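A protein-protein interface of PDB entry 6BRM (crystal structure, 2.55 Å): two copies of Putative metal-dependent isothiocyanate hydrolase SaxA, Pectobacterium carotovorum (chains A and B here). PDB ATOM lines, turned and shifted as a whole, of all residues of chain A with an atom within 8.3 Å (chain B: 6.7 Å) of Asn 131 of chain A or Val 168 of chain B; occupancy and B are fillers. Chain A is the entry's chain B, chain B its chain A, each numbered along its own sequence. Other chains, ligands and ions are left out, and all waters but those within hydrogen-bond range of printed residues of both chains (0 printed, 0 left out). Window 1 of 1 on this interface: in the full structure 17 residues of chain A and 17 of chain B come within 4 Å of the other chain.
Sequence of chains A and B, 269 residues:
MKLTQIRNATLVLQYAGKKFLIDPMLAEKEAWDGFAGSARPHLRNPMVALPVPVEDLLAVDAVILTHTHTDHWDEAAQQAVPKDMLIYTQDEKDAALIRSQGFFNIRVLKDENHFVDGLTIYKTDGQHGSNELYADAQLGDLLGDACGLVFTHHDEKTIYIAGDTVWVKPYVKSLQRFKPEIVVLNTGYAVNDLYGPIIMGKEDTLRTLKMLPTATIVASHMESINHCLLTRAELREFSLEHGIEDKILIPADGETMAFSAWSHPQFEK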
ATOM      1  N   ASP A 125      15.176   7.202   6.317  1.00  0.00           N
ATOM      2  CA  ASP A 125      15.500   7.592   4.942  1.00  0.00           C
ATOM      3  C   ASP A 125      16.975   7.327   4.680  1.00  0.00           C
ATOM      4  O   ASP A 125      17.824   7.798   5.425  1.00  0.00           O
ATOM      5  CB  ASP A 125      15.177   9.072   4.687  1.00  0.00           C
ATOM      6  CG  ASP A 125      15.193   9.434   3.195  1.00  0.00           C
ATOM      7  OD1 ASP A 125      14.463   8.796   2.409  1.00  0.00           O
ATOM      8  OD2 ASP A 125      15.932  10.363   2.808  1.00  0.00           O
ATOM      9  N   GLN A 127      20.050   6.639   1.264  1.00  0.00           N
ATOM     10  CA  GLN A 127      20.341   6.976  -0.123  1.00  0.00           C
ATOM     11  C   GLN A 127      21.006   5.783  -0.810  1.00  0.00           C
ATOM     12  O   GLN A 127      22.134   5.421  -0.477  1.00  0.00           O
ATOM     13  CB  GLN A 127      21.225   8.220  -0.199  1.00  0.00           C
ATOM     14  CG  GLN A 127      21.210   8.894  -1.563  1.00  0.00           C
ATOM     15  CD  GLN A 127      21.770  10.300  -1.529  1.00  0.00           C
ATOM     16  OE1 GLN A 127      21.021  11.276  -1.471  1.00  0.00           O
ATOM     17  NE2 GLN A 127      23.093  10.410  -1.557  1.00  0.00           N
ATOM     18  N   HIS A 128      20.303   5.193  -1.778  1.00  0.00           N
ATOM     19  CA  HIS A 128      20.738   3.976  -2.472  1.00  0.00           C
ATOM     20  C   HIS A 128      21.652   4.349  -3.647  1.00  0.00           C
ATOM     21  O   HIS A 128      21.352   4.057  -4.806  1.00  0.00           O
ATOM     22  CB  HIS A 128      19.498   3.195  -2.948  1.00  0.00           C
ATOM     23  CG  HIS A 128      19.740   1.739  -3.208  1.00  0.00           C
ATOM     24  ND1 HIS A 128      20.993   1.211  -3.432  1.00  0.00           N
ATOM     25  CD2 HIS A 128      18.872   0.703  -3.307  1.00  0.00           C
ATOM     26  CE1 HIS A 128      20.888  -0.090  -3.644  1.00  0.00           C
ATOM     27  NE2 HIS A 128      19.612  -0.422  -3.582  1.00  0.00           N
ATOM     28  N   GLY A 129      22.783   4.979  -3.339  1.00  0.00           N
ATOM     29  CA  GLY A 129      23.673   5.530  -4.364  1.00  0.00           C
ATOM     30  C   GLY A 129      24.401   6.771  -3.900  1.00  0.00           C
ATOM     31  O   GLY A 129      24.073   7.344  -2.863  1.00  0.00           O
ATOM     32  N   SER A 130      25.396   7.179  -4.683  1.00  0.00           N
ATOM     33  CA  SER A 130      26.154   8.409  -4.431  1.00  0.00           C
ATOM     34  C   SER A 130      25.331   9.650  -4.773  1.00  0.00           C
ATOM     35  O   SER A 130      24.304   9.555  -5.440  1.00  0.00           O
ATOM     36  CB  SER A 130      27.431   8.417  -5.269  1.00  0.00           C
ATOM     37  OG  SER A 130      27.116   8.398  -6.654  1.00  0.00           O
ATOM     38  N   ASN A 131      25.804  10.809  -4.326  1.00  0.00           N
ATOM     39  CA  ASN A 131      25.182  12.103  -4.652  1.00  0.00           C
ATOM     40  C   ASN A 131      25.087  12.352  -6.157  1.00  0.00           C
ATOM     41  O   ASN A 131      24.092  12.904  -6.632  1.00  0.00           O
ATOM     42  CB  ASN A 131      25.961  13.256  -4.000  1.00  0.00           C
ATOM     43  CG  ASN A 131      25.755  13.332  -2.499  1.00  0.00           C
ATOM     44  OD1 ASN A 131      25.094  12.485  -1.905  1.00  0.00           O
ATOM     45  ND2 ASN A 131      26.323  14.357  -1.879  1.00  0.00           N
ATOM     46  N   GLU A 132      26.118  11.933  -6.891  1.00  0.00           N
ATOM     47  CA  GLU A 132      26.191  12.146  -8.343  1.00  0.00           C
ATOM     48  C   GLU A 132      25.124  11.319  -9.054  1.00  0.00           C
ATOM     49  O   GLU A 132      24.403  11.834  -9.912  1.00  0.00           O
ATOM     50  CB  GLU A 132      27.579  11.784  -8.910  1.00  0.00           C
ATOM     51  CG  GLU A 132      28.807  12.291  -8.144  1.00  0.00           C
ATOM     52  CD  GLU A 132      28.685  13.725  -7.648  1.00  0.00           C
ATOM     53  OE1 GLU A 132      28.198  14.591  -8.411  1.00  0.00           O
ATOM     54  OE2 GLU A 132      29.088  13.984  -6.493  1.00  0.00           O
ATOM     55  N   LEU A 133      25.020  10.047  -8.671  1.00  0.00           N
ATOM     56  CA  LEU A 133      24.014   9.131  -9.218  1.00  0.00           C
ATOM     57  C   LEU A 133      22.596   9.706  -9.213  1.00  0.00           C
ATOM     58  O   LEU A 133      21.865   9.541 -10.187  1.00  0.00           O
ATOM     59  CB  LEU A 133      24.033   7.798  -8.458  1.00  0.00           C
ATOM     60  CG  LEU A 133      23.134   6.680  -9.014  1.00  0.00           C
ATOM     61  CD1 LEU A 133      23.859   5.337  -9.022  1.00  0.00           C
ATOM     62  CD2 LEU A 133      21.817   6.567  -8.256  1.00  0.00           C
ATOM     63  N   TYR A 134      22.213  10.377  -8.129  1.00  0.00           N
ATOM     64  CA  TYR A 134      20.862  10.961  -8.010  1.00  0.00           C
ATOM     65  C   TYR A 134      20.656  12.290  -8.765  1.00  0.00           C
ATOM     66  O   TYR A 134      19.526  12.779  -8.841  1.00  0.00           O
ATOM     67  CB  TYR A 134      20.446  11.076  -6.537  1.00  0.00           C
ATOM     68  CG  TYR A 134      20.042   9.746  -5.943  1.00  0.00           C
ATOM     69  CD1 TYR A 134      18.755   9.251  -6.116  1.00  0.00           C
ATOM     70  CD2 TYR A 134      20.955   8.969  -5.230  1.00  0.00           C
ATOM     71  CE1 TYR A 134      18.383   8.024  -5.588  1.00  0.00           C
ATOM     72  CE2 TYR A 134      20.593   7.740  -4.694  1.00  0.00           C
ATOM     73  CZ  TYR A 134      19.307   7.274  -4.871  1.00  0.00           C
ATOM     74  OH  TYR A 134      18.943   6.060  -4.334  1.00  0.00           O
ATOM     75  N   ALA A 135      21.727  12.866  -9.314  1.00  0.00           N
ATOM     76  CA  ALA A 135      21.611  13.950 -10.307  1.00  0.00           C
ATOM     77  C   ALA A 135      21.074  13.429 -11.648  1.00  0.00           C
ATOM     78  O   ALA A 135      20.432  14.176 -12.396  1.00  0.00           O
ATOM     79  CB  ALA A 135      22.949  14.646 -10.512  1.00  0.00           C
ATOM     80  N   ASP A 136      21.357  12.159 -11.948  1.00  0.00           N
ATOM     81  CA  ASP A 136      20.782  11.468 -13.102  1.00  0.00           C
ATOM     82  C   ASP A 136      19.345  11.089 -12.758  1.00  0.00           C
ATOM     83  O   ASP A 136      19.113  10.300 -11.842  1.00  0.00           O
ATOM     84  CB  ASP A 136      21.611  10.218 -13.444  1.00  0.00           C
ATOM     85  CG  ASP A 136      21.210   9.578 -14.769  1.00  0.00           C
ATOM     86  OD1 ASP A 136      20.053   9.119 -14.903  1.00  0.00           O
ATOM     87  OD2 ASP A 136      22.068   9.506 -15.672  1.00  0.00           O
ATOM     88  N   VAL A 166      24.025   4.041   1.094  1.00  0.00           N
ATOM     89  CA  VAL A 166      25.430   4.397   1.340  1.00  0.00           C
ATOM     90  C   VAL A 166      25.472   5.407   2.494  1.00  0.00           C
ATOM     91  O   VAL A 166      24.422   5.792   3.033  1.00  0.00           O
ATOM     92  CB  VAL A 166      26.156   4.952   0.079  1.00  0.00           C
ATOM     93  CG1 VAL A 166      25.963   4.018  -1.110  1.00  0.00           C
ATOM     94  CG2 VAL A 166      25.719   6.376  -0.269  1.00  0.00           C
ATOM     95  N   TRP A 167      26.676   5.823   2.878  1.00  0.00           N
ATOM     96  CA  TRP A 167      26.840   6.800   3.954  1.00  0.00           C
ATOM     97  C   TRP A 167      26.303   8.181   3.544  1.00  0.00           C
ATOM     98  O   TRP A 167      26.901   8.875   2.716  1.00  0.00           O
ATOM     99  CB  TRP A 167      28.308   6.902   4.383  1.00  0.00           C
ATOM    100  CG  TRP A 167      28.509   7.678   5.649  1.00  0.00           C
ATOM    101  CD1 TRP A 167      28.448   9.035   5.801  1.00  0.00           C
ATOM    102  CD2 TRP A 167      28.816   7.145   6.943  1.00  0.00           C
ATOM    103  NE1 TRP A 167      28.691   9.377   7.109  1.00  0.00           N
ATOM    104  CE2 TRP A 167      28.918   8.237   7.833  1.00  0.00           C
ATOM    105  CE3 TRP A 167      29.008   5.850   7.439  1.00  0.00           C
ATOM    106  CZ2 TRP A 167      29.214   8.077   9.190  1.00  0.00           C
ATOM    107  CZ3 TRP A 167      29.293   5.689   8.789  1.00  0.00           C
ATOM    108  CH2 TRP A 167      29.395   6.799   9.651  1.00  0.00           C
ATOM    109  N   VAL A 168      25.159   8.548   4.127  1.00  0.00           N
ATOM    110  CA  VAL A 168      24.628   9.918   4.076  1.00  0.00           C
ATOM    111  C   VAL A 168      24.295  10.357   5.503  1.00  0.00           C
ATOM    112  O   VAL A 168      24.298   9.526   6.409  1.00  0.00           O
ATOM    113  CB  VAL A 168      23.407  10.031   3.140  1.00  0.00           C
ATOM    114  CG1 VAL A 168      23.858   9.951   1.697  1.00  0.00           C
ATOM    115  CG2 VAL A 168      22.361   8.953   3.421  1.00  0.00           C
ATOM    116  N   LYS A 169      24.022  11.644   5.715  1.00  0.00           N
ATOM    117  CA  LYS A 169      23.799  12.151   7.090  1.00  0.00           C
ATOM    118  C   LYS A 169      22.480  11.681   7.736  1.00  0.00           C
ATOM    119  O   LYS A 169      22.421  11.576   8.961  1.00  0.00           O
ATOM    120  CB  LYS A 169      23.981  13.684   7.190  1.00  0.00           C
ATOM    121  CG  LYS A 169      22.738  14.526   7.470  1.00  0.00           C
ATOM    122  CD  LYS A 169      23.106  15.999   7.533  1.00  0.00           C
ATOM    123  CE  LYS A 169      21.926  16.859   7.942  1.00  0.00           C
ATOM    124  NZ  LYS A 169      20.775  16.761   7.009  1.00  0.00           N
ATOM    125  N   PRO A 170      21.427  11.398   6.935  1.00  0.00           N
ATOM    126  CA  PRO A 170      20.248  10.745   7.528  1.00  0.00           C
ATOM    127  C   PRO A 170      20.536   9.400   8.211  1.00  0.00           C
ATOM    128  O   PRO A 170      19.811   9.009   9.135  1.00  0.00           O
ATOM    129  CB  PRO A 170      19.322  10.555   6.326  1.00  0.00           C
ATOM    130  CG  PRO A 170      19.650  11.702   5.446  1.00  0.00           C
ATOM    131  CD  PRO A 170      21.145  11.833   5.554  1.00  0.00           C
ATOM    132  N   TYR A 195      29.337   5.818 -11.330  1.00  0.00           N
ATOM    133  CA  TYR A 195      28.907   6.637 -10.179  1.00  0.00           C
ATOM    134  C   TYR A 195      29.300   6.090  -8.790  1.00  0.00           C
ATOM    135  O   TYR A 195      28.809   6.580  -7.771  1.00  0.00           O
ATOM    136  CB  TYR A 195      27.390   6.882 -10.252  1.00  0.00           C
ATOM    137  CG  TYR A 195      26.969   7.753 -11.421  1.00  0.00           C
ATOM    138  CD1 TYR A 195      27.345   9.097 -11.483  1.00  0.00           C
ATOM    139  CD2 TYR A 195      26.184   7.244 -12.457  1.00  0.00           C
ATOM    140  CE1 TYR A 195      26.961   9.907 -12.544  1.00  0.00           C
ATOM    141  CE2 TYR A 195      25.796   8.047 -13.523  1.00  0.00           C
ATOM    142  CZ  TYR A 195      26.186   9.376 -13.561  1.00  0.00           C
ATOM    143  OH  TYR A 195      25.805  10.173 -14.616  1.00  0.00           O
ATOM    144  N   PRO A 197      30.054   3.324  -5.464  1.00  0.00           N
ATOM    145  CA  PRO A 197      29.245   2.394  -4.657  1.00  0.00           C
ATOM    146  C   PRO A 197      27.766   2.773  -4.501  1.00  0.00           C
ATOM    147  O   PRO A 197      27.441   3.960  -4.396  1.00  0.00           O
ATOM    148  CB  PRO A 197      29.944   2.410  -3.294  1.00  0.00           C
ATOM    149  CG  PRO A 197      31.359   2.742  -3.605  1.00  0.00           C
ATOM    150  CD  PRO A 197      31.307   3.689  -4.771  1.00  0.00           C
ATOM    151  N   ASP B 125      14.704  18.986   4.210  1.00  0.00           N
ATOM    152  CA  ASP B 125      16.039  18.572   4.622  1.00  0.00           C
ATOM    153  C   ASP B 125      17.041  18.852   3.503  1.00  0.00           C
ATOM    154  O   ASP B 125      16.667  18.975   2.341  1.00  0.00           O
ATOM    155  CB  ASP B 125      16.036  17.078   4.992  1.00  0.00           C
ATOM    156  CG  ASP B 125      17.382  16.592   5.550  1.00  0.00           C
ATOM    157  OD1 ASP B 125      18.079  17.376   6.237  1.00  0.00           O
ATOM    158  OD2 ASP B 125      17.743  15.420   5.294  1.00  0.00           O
ATOM    159  N   GLY B 126      18.306  18.990   3.878  1.00  0.00           N
ATOM    160  CA  GLY B 126      19.419  19.053   2.935  1.00  0.00           C
ATOM    161  C   GLY B 126      20.642  18.398   3.544  1.00  0.00           C
ATOM    162  O   GLY B 126      20.543  17.726   4.569  1.00  0.00           O
ATOM    163  N   GLN B 127      21.789  18.575   2.902  1.00  0.00           N
ATOM    164  CA  GLN B 127      23.065  18.093   3.426  1.00  0.00           C
ATOM    165  C   GLN B 127      24.126  19.144   3.138  1.00  0.00           C
ATOM    166  O   GLN B 127      24.417  19.435   1.983  1.00  0.00           O
ATOM    167  CB  GLN B 127      23.443  16.750   2.797  1.00  0.00           C
ATOM    168  CG  GLN B 127      24.600  16.048   3.492  1.00  0.00           C
ATOM    169  CD  GLN B 127      24.837  14.633   2.984  1.00  0.00           C
ATOM    170  OE1 GLN B 127      23.915  13.815   2.929  1.00  0.00           O
ATOM    171  NE2 GLN B 127      26.081  14.332   2.624  1.00  0.00           N
ATOM    172  N   HIS B 128      24.706  19.698   4.200  1.00  0.00           N
ATOM    173  CA  HIS B 128      25.590  20.853   4.117  1.00  0.00           C
ATOM    174  C   HIS B 128      27.043  20.371   4.051  1.00  0.00           C
ATOM    175  O   HIS B 128      27.874  20.714   4.896  1.00  0.00           O
ATOM    176  CB  HIS B 128      25.331  21.751   5.329  1.00  0.00           C
ATOM    177  CG  HIS B 128      25.917  23.122   5.216  1.00  0.00           C
ATOM    178  ND1 HIS B 128      26.902  23.445   4.307  1.00  0.00           N
ATOM    179  CD2 HIS B 128      25.677  24.247   5.928  1.00  0.00           C
ATOM    180  CE1 HIS B 128      27.235  24.715   4.458  1.00  0.00           C
ATOM    181  NE2 HIS B 128      26.511  25.223   5.440  1.00  0.00           N
ATOM    182  N   GLY B 129      27.342  19.587   3.018  1.00  0.00           N
ATOM    183  CA  GLY B 129      28.622  18.891   2.899  1.00  0.00           C
ATOM    184  C   GLY B 129      28.483  17.620   2.083  1.00  0.00           C
ATOM    185  O   GLY B 129      27.375  17.167   1.812  1.00  0.00           O
ATOM    186  N   SER B 130      29.615  17.043   1.695  1.00  0.00           N
ATOM    187  CA  SER B 130      29.626  15.808   0.912  1.00  0.00           C
ATOM    188  C   SER B 130      29.370  14.610   1.814  1.00  0.00           C
ATOM    189  O   SER B 130      29.436  14.723   3.038  1.00  0.00           O
ATOM    190  CB  SER B 130      30.972  15.641   0.201  1.00  0.00           C
ATOM    191  OG  SER B 130      32.042  15.622   1.129  1.00  0.00           O
ATOM    192  N   ASN B 131      29.100  13.462   1.198  1.00  0.00           N
ATOM    193  CA  ASN B 131      29.003  12.180   1.918  1.00  0.00           C
ATOM    194  C   ASN B 131      30.303  11.847   2.675  1.00  0.00           C
ATOM    195  O   ASN B 131      30.271  11.215   3.735  1.00  0.00           O
ATOM    196  CB  ASN B 131      28.650  11.044   0.942  1.00  0.00           C
ATOM    197  CG  ASN B 131      27.238  11.168   0.366  1.00  0.00           C
ATOM    198  OD1 ASN B 131      26.481  12.070   0.726  1.00  0.00           O
ATOM    199  ND2 ASN B 131      26.883  10.255  -0.535  1.00  0.00           N
ATOM    200  N   THR B 165      22.783  23.454   1.106  1.00  0.00           N
ATOM    201  CA  THR B 165      22.774  22.020   0.821  1.00  0.00           C
ATOM    202  C   THR B 165      23.481  21.741  -0.506  1.00  0.00           C
ATOM    203  O   THR B 165      23.436  22.573  -1.409  1.00  0.00           O
ATOM    204  CB  THR B 165      21.331  21.469   0.778  1.00  0.00           C
ATOM    205  OG1 THR B 165      21.360  20.045   0.625  1.00  0.00           O
ATOM    206  CG2 THR B 165      20.515  22.084  -0.368  1.00  0.00           C
ATOM    207  N   VAL B 166      24.156  20.595  -0.603  1.00  0.00           N
ATOM    208  CA  VAL B 166      24.672  20.095  -1.893  1.00  0.00           C
ATOM    209  C   VAL B 166      23.610  19.198  -2.506  1.00  0.00           C
ATOM    210  O   VAL B 166      22.565  18.964  -1.885  1.00  0.00           O
ATOM    211  CB  VAL B 166      26.022  19.335  -1.770  1.00  0.00           C
ATOM    212  CG1 VAL B 166      27.074  20.232  -1.130  1.00  0.00           C
ATOM    213  CG2 VAL B 166      25.883  18.011  -1.010  1.00  0.00           C
ATOM    214  N   TRP B 167      23.865  18.706  -3.718  1.00  0.00           N
ATOM    215  CA  TRP B 167      22.925  17.799  -4.376  1.00  0.00           C
ATOM    216  C   TRP B 167      22.858  16.484  -3.601  1.00  0.00           C
ATOM    217  O   TRP B 167      23.834  15.736  -3.542  1.00  0.00           O
ATOM    218  CB  TRP B 167      23.302  17.533  -5.841  1.00  0.00           C
ATOM    219  CG  TRP B 167      22.153  16.977  -6.632  1.00  0.00           C
ATOM    220  CD1 TRP B 167      21.709  15.685  -6.641  1.00  0.00           C
ATOM    221  CD2 TRP B 167      21.285  17.705  -7.507  1.00  0.00           C
ATOM    222  NE1 TRP B 167      20.620  15.564  -7.469  1.00  0.00           N
ATOM    223  CE2 TRP B 167      20.339  16.787  -8.015  1.00  0.00           C
ATOM    224  CE3 TRP B 167      21.221  19.044  -7.919  1.00  0.00           C
ATOM    225  CZ2 TRP B 167      19.343  17.160  -8.913  1.00  0.00           C
ATOM    226  CZ3 TRP B 167      20.222  19.419  -8.811  1.00  0.00           C
ATOM    227  CH2 TRP B 167      19.293  18.477  -9.294  1.00  0.00           C
ATOM    228  N   VAL B 168      21.712  16.252  -2.972  1.00  0.00           N
ATOM    229  CA  VAL B 168      21.392  14.981  -2.323  1.00  0.00           C
ATOM    230  C   VAL B 168      19.953  14.634  -2.688  1.00  0.00           C
ATOM    231  O   VAL B 168      19.231  15.475  -3.238  1.00  0.00           O
ATOM    232  CB  VAL B 168      21.583  15.030  -0.783  1.00  0.00           C
ATOM    233  CG1 VAL B 168      23.042  14.818  -0.410  1.00  0.00           C
ATOM    234  CG2 VAL B 168      21.071  16.337  -0.194  1.00  0.00           C
ATOM    235  N   LYS B 169      19.545  13.400  -2.399  1.00  0.00           N
ATOM    236  CA  LYS B 169      18.210  12.923  -2.763  1.00  0.00           C
ATOM    237  C   LYS B 169      17.070  13.745  -2.154  1.00  0.00           C
ATOM    238  O   LYS B 169      16.124  14.061  -2.864  1.00  0.00           O
ATOM    239  CB  LYS B 169      18.048  11.435  -2.433  1.00  0.00           C
ATOM    240  CG  LYS B 169      16.670  10.863  -2.749  1.00  0.00           C
ATOM    241  CD  LYS B 169      16.630   9.348  -2.637  1.00  0.00           C
ATOM    242  CE  LYS B 169      16.852   8.873  -1.210  1.00  0.00           C
ATOM    243  NZ  LYS B 169      16.731   7.395  -1.109  1.00  0.00           N
ATOM    244  N   PRO B 170      17.144  14.098  -0.852  1.00  0.00           N
ATOM    245  CA  PRO B 170      16.098  14.961  -0.278  1.00  0.00           C
ATOM    246  C   PRO B 170      15.797  16.249  -1.054  1.00  0.00           C
ATOM    247  O   PRO B 170      14.652  16.710  -1.028  1.00  0.00           O
ATOM    248  CB  PRO B 170      16.642  15.287   1.112  1.00  0.00           C
ATOM    249  CG  PRO B 170      17.410  14.067   1.479  1.00  0.00           C
ATOM    250  CD  PRO B 170      18.042  13.583   0.203  1.00  0.00           C
ATOM    251  N   TYR B 171      16.800  16.818  -1.725  1.00  0.00           N
ATOM    252  CA  TYR B 171      16.585  17.948  -2.635  1.00  0.00           C
ATOM    253  C   TYR B 171      15.786  17.514  -3.866  1.00  0.00           C
ATOM    254  O   TYR B 171      14.881  18.228  -4.297  1.00  0.00           O
ATOM    255  CB  TYR B 171      17.920  18.589  -3.055  1.00  0.00           C
ATOM    256  CG  TYR B 171      17.770  19.685  -4.089  1.00  0.00           C
ATOM    257  CD1 TYR B 171      17.364  20.973  -3.723  1.00  0.00           C
ATOM    258  CD2 TYR B 171      18.016  19.433  -5.439  1.00  0.00           C
ATOM    259  CE1 TYR B 171      17.215  21.978  -4.673  1.00  0.00           C
ATOM    260  CE2 TYR B 171      17.868  20.429  -6.394  1.00  0.00           C
ATOM    261  CZ  TYR B 171      17.470  21.698  -6.011  1.00  0.00           C
ATOM    262  OH  TYR B 171      17.328  22.672  -6.969  1.00  0.00           O
ATOM    263  N   VAL B 172      16.130  16.353  -4.425  1.00  0.00           N
ATOM    264  CA  VAL B 172      15.408  15.774  -5.575  1.00  0.00           C
ATOM    265  C   VAL B 172      13.937  15.478  -5.243  1.00  0.00           C
ATOM    266  O   VAL B 172      13.042  15.846  -6.015  1.00  0.00           O
ATOM    267  CB  VAL B 172      16.119  14.500  -6.121  1.00  0.00           C
ATOM    268  CG1 VAL B 172      15.246  13.729  -7.108  1.00  0.00           C
ATOM    269  CG2 VAL B 172      17.435  14.876  -6.781  1.00  0.00           C
ATOM    270  N   LYS B 173      13.695  14.811  -4.114  1.00  0.00           N
ATOM    271  CA  LYS B 173      12.321  14.509  -3.668  1.00  0.00           C
ATOM    272  C   LYS B 173      11.492  15.764  -3.364  1.00  0.00           C
ATOM    273  O   LYS B 173      10.274  15.751  -3.537  1.00  0.00           O
ATOM    274  CB  LYS B 173      12.314  13.577  -2.443  1.00  0.00           C
ATOM    275  CG  LYS B 173      12.453  12.095  -2.773  1.00  0.00           C
ATOM    276  CD  LYS B 173      12.348  11.236  -1.518  1.00  0.00           C
ATOM    277  CE  LYS B 173      13.645  11.245  -0.714  1.00  0.00           C
ATOM    278  NZ  LYS B 173      13.458  11.261   0.764  1.00  0.00           N
ATOM    279  N   MET B 200      26.045  24.228  -3.155  1.00  0.00           N
ATOM    280  CA  MET B 200      25.913  24.087  -4.611  1.00  0.00           C
ATOM    281  C   MET B 200      26.754  25.067  -5.429  1.00  0.00           C
ATOM    282  O   MET B 200      27.336  26.017  -4.896  1.00  0.00           O
ATOM    283  CB  MET B 200      24.437  24.200  -5.019  1.00  0.00           C
ATOM    284  CG  MET B 200      23.627  22.973  -4.645  1.00  0.00           C
ATOM    285  SD  MET B 200      21.850  23.208  -4.756  1.00  0.00           S
ATOM    286  CE  MET B 200      21.321  21.503  -4.902  1.00  0.00           C
ATOM    287  N   ARG B 207      21.501  20.638 -13.522  1.00  0.00           N
ATOM    288  CA  ARG B 207      20.866  19.430 -12.976  1.00  0.00           C
ATOM    289  C   ARG B 207      19.401  19.650 -12.568  1.00  0.00           C
ATOM    290  O   ARG B 207      18.565  18.775 -12.800  1.00  0.00           O
ATOM    291  CB  ARG B 207      21.643  18.912 -11.757  1.00  0.00           C
ATOM    292  CG  ARG B 207      23.006  18.291 -12.021  1.00  0.00           C
ATOM    293  CD  ARG B 207      23.750  18.161 -10.699  1.00  0.00           C
ATOM    294  NE  ARG B 207      25.054  17.511 -10.797  1.00  0.00           N
ATOM    295  CZ  ARG B 207      25.927  17.394  -9.789  1.00  0.00           C
ATOM    296  NH1 ARG B 207      25.653  17.885  -8.578  1.00  0.00           N
ATOM    297  NH2 ARG B 207      27.093  16.782  -9.989  1.00  0.00           N
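OD1 of Asp 125 of chain B lies within salt-bridge range of NZ of Lys 169 of chain A (2.9 Å).
The backbone carbonyl oxygen of Gly 126 of chain B is in hydrogen-bond range of the side-chain amino group of Lys 169 of chain A.
OD1 of Asn 131 of chain A lies close to OD1 of Asn 131 of chain B (3.0 Å).
The backbone carbonyl oxygen of Trp 167 of chain B lies close to the side-chain amide nitrogen of Asn 131 of chain A, 3.3 Å away.
O of Tyr 134 of chain A lies within hydrogen-bond range of NE1 of Trp 167 of chain B (3.3 Å).
OE1 of Gln 127 of chain A lies within hydrogen-bond range of N of Lys 169 of chain B (2.7 Å).
OD1 of Asp 125 of chain A lies within salt-bridge range of NZ of Lys 173 of chain B, at 3.1 Å.
The side-chain carboxylate of Glu 132 of chain A is in salt-bridge range of the guanidinium group of Arg 207 of chain B, 2.9 Å away.
The backbone NH of Ala 135 of chain A lies close to the indole nitrogen of Trp 167 of chain B, 3.5 Å away.
The backbone NH (N) of Gln 127 of chain B lies within hydrogen-bond range of the side-chain hydroxyl (OG1) of Thr 165 of chain B, 2.7 Å away.
The backbone carbonyl oxygen (O) of Gln 127 of chain B is in hydrogen-bond range of the backbone NH (N) of Val 166 of chain B, 2.8 Å away.
NE2 of Gln 127 of chain A sits at hydrogen-bond distance from O of Gly 129 of chain A (3.5 Å).
The side-chain amide nitrogen of Gln 127 of chain A sits at hydrogen-bond distance from the side-chain amide oxygen of Asn 131 of chain A, 2.9 Å away.
C of Val 168 of chain B touches OE1 of Gln 127 of chain A (3.7 Å).
Asn 131 of chain A touches Val 168 of chain B.
Tyr 134 of chain A touches Lys 169 of chain B (CE1 to CD, 3.7 Å).
Tyr 134 of chain A touches Val 172 of chain B.
CB of Ala 135 of chain A touches NE of Arg 207 of chain B (3.6 Å).
CB of Val 168 of chain A touches OE1 of Gln 127 of chain B, at 3.8 Å.
Val 168 of chain A touches Asn 131 of chain B (CG1 to OD1, 3.5 Å).
Lys 169 of chain A touches Gln 127 of chain B (N to OE1, 3.5 Å).
Of chain B, only Asn 131, Val 166, Trp 167 and Val 168 come within 4 Å of Asn 131 of chain A.
Of the printed residues of chain B, Glu 132 of chain A touches Arg 207.
Asp 136 of chain A touches none of the printed residues of chain B.
His 128 of chain B touches none of the printed residues of chain A.
Val 168 of chain B touches just these residues of chain A: Gln 127 (3.7 Å) and Asn 131 (3.4 Å).
Of the printed residues of chain A, Lys 173 of chain B touches Asp 125 (3.1 Å).
Hydrophobic or aromatic side chains of chain A that line the printed part of chain B: Tyr 134, Ala 135, Trp 167 and Val 168.
Of the 18 printed residues of chain B, 11 touch a printed residue of chain A.
Hydrophobic or aromatic side chains of chain B within 4 Å of the printed part of chain A: Val 166, Trp 167, Val 168 and Val 172.
Among the printed residues, 20 pairs touch across the chains.
Gln 127 of chain A touches Lys 169 of chain B, and with the chains exchanged Lys 169 of chain A touches Gln 127 of chain B.
Asn 131 of chain B touches its own counterpart, Asn 131 of chain A.
Positions printed for both chains: 125, 127, 128, 129, 130, 131, 166, 167, 168, 169 and 170.
Of the 20 pairs that touch across the chains among the printed residues, 9 have their exchanged pair printed and touching as well.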
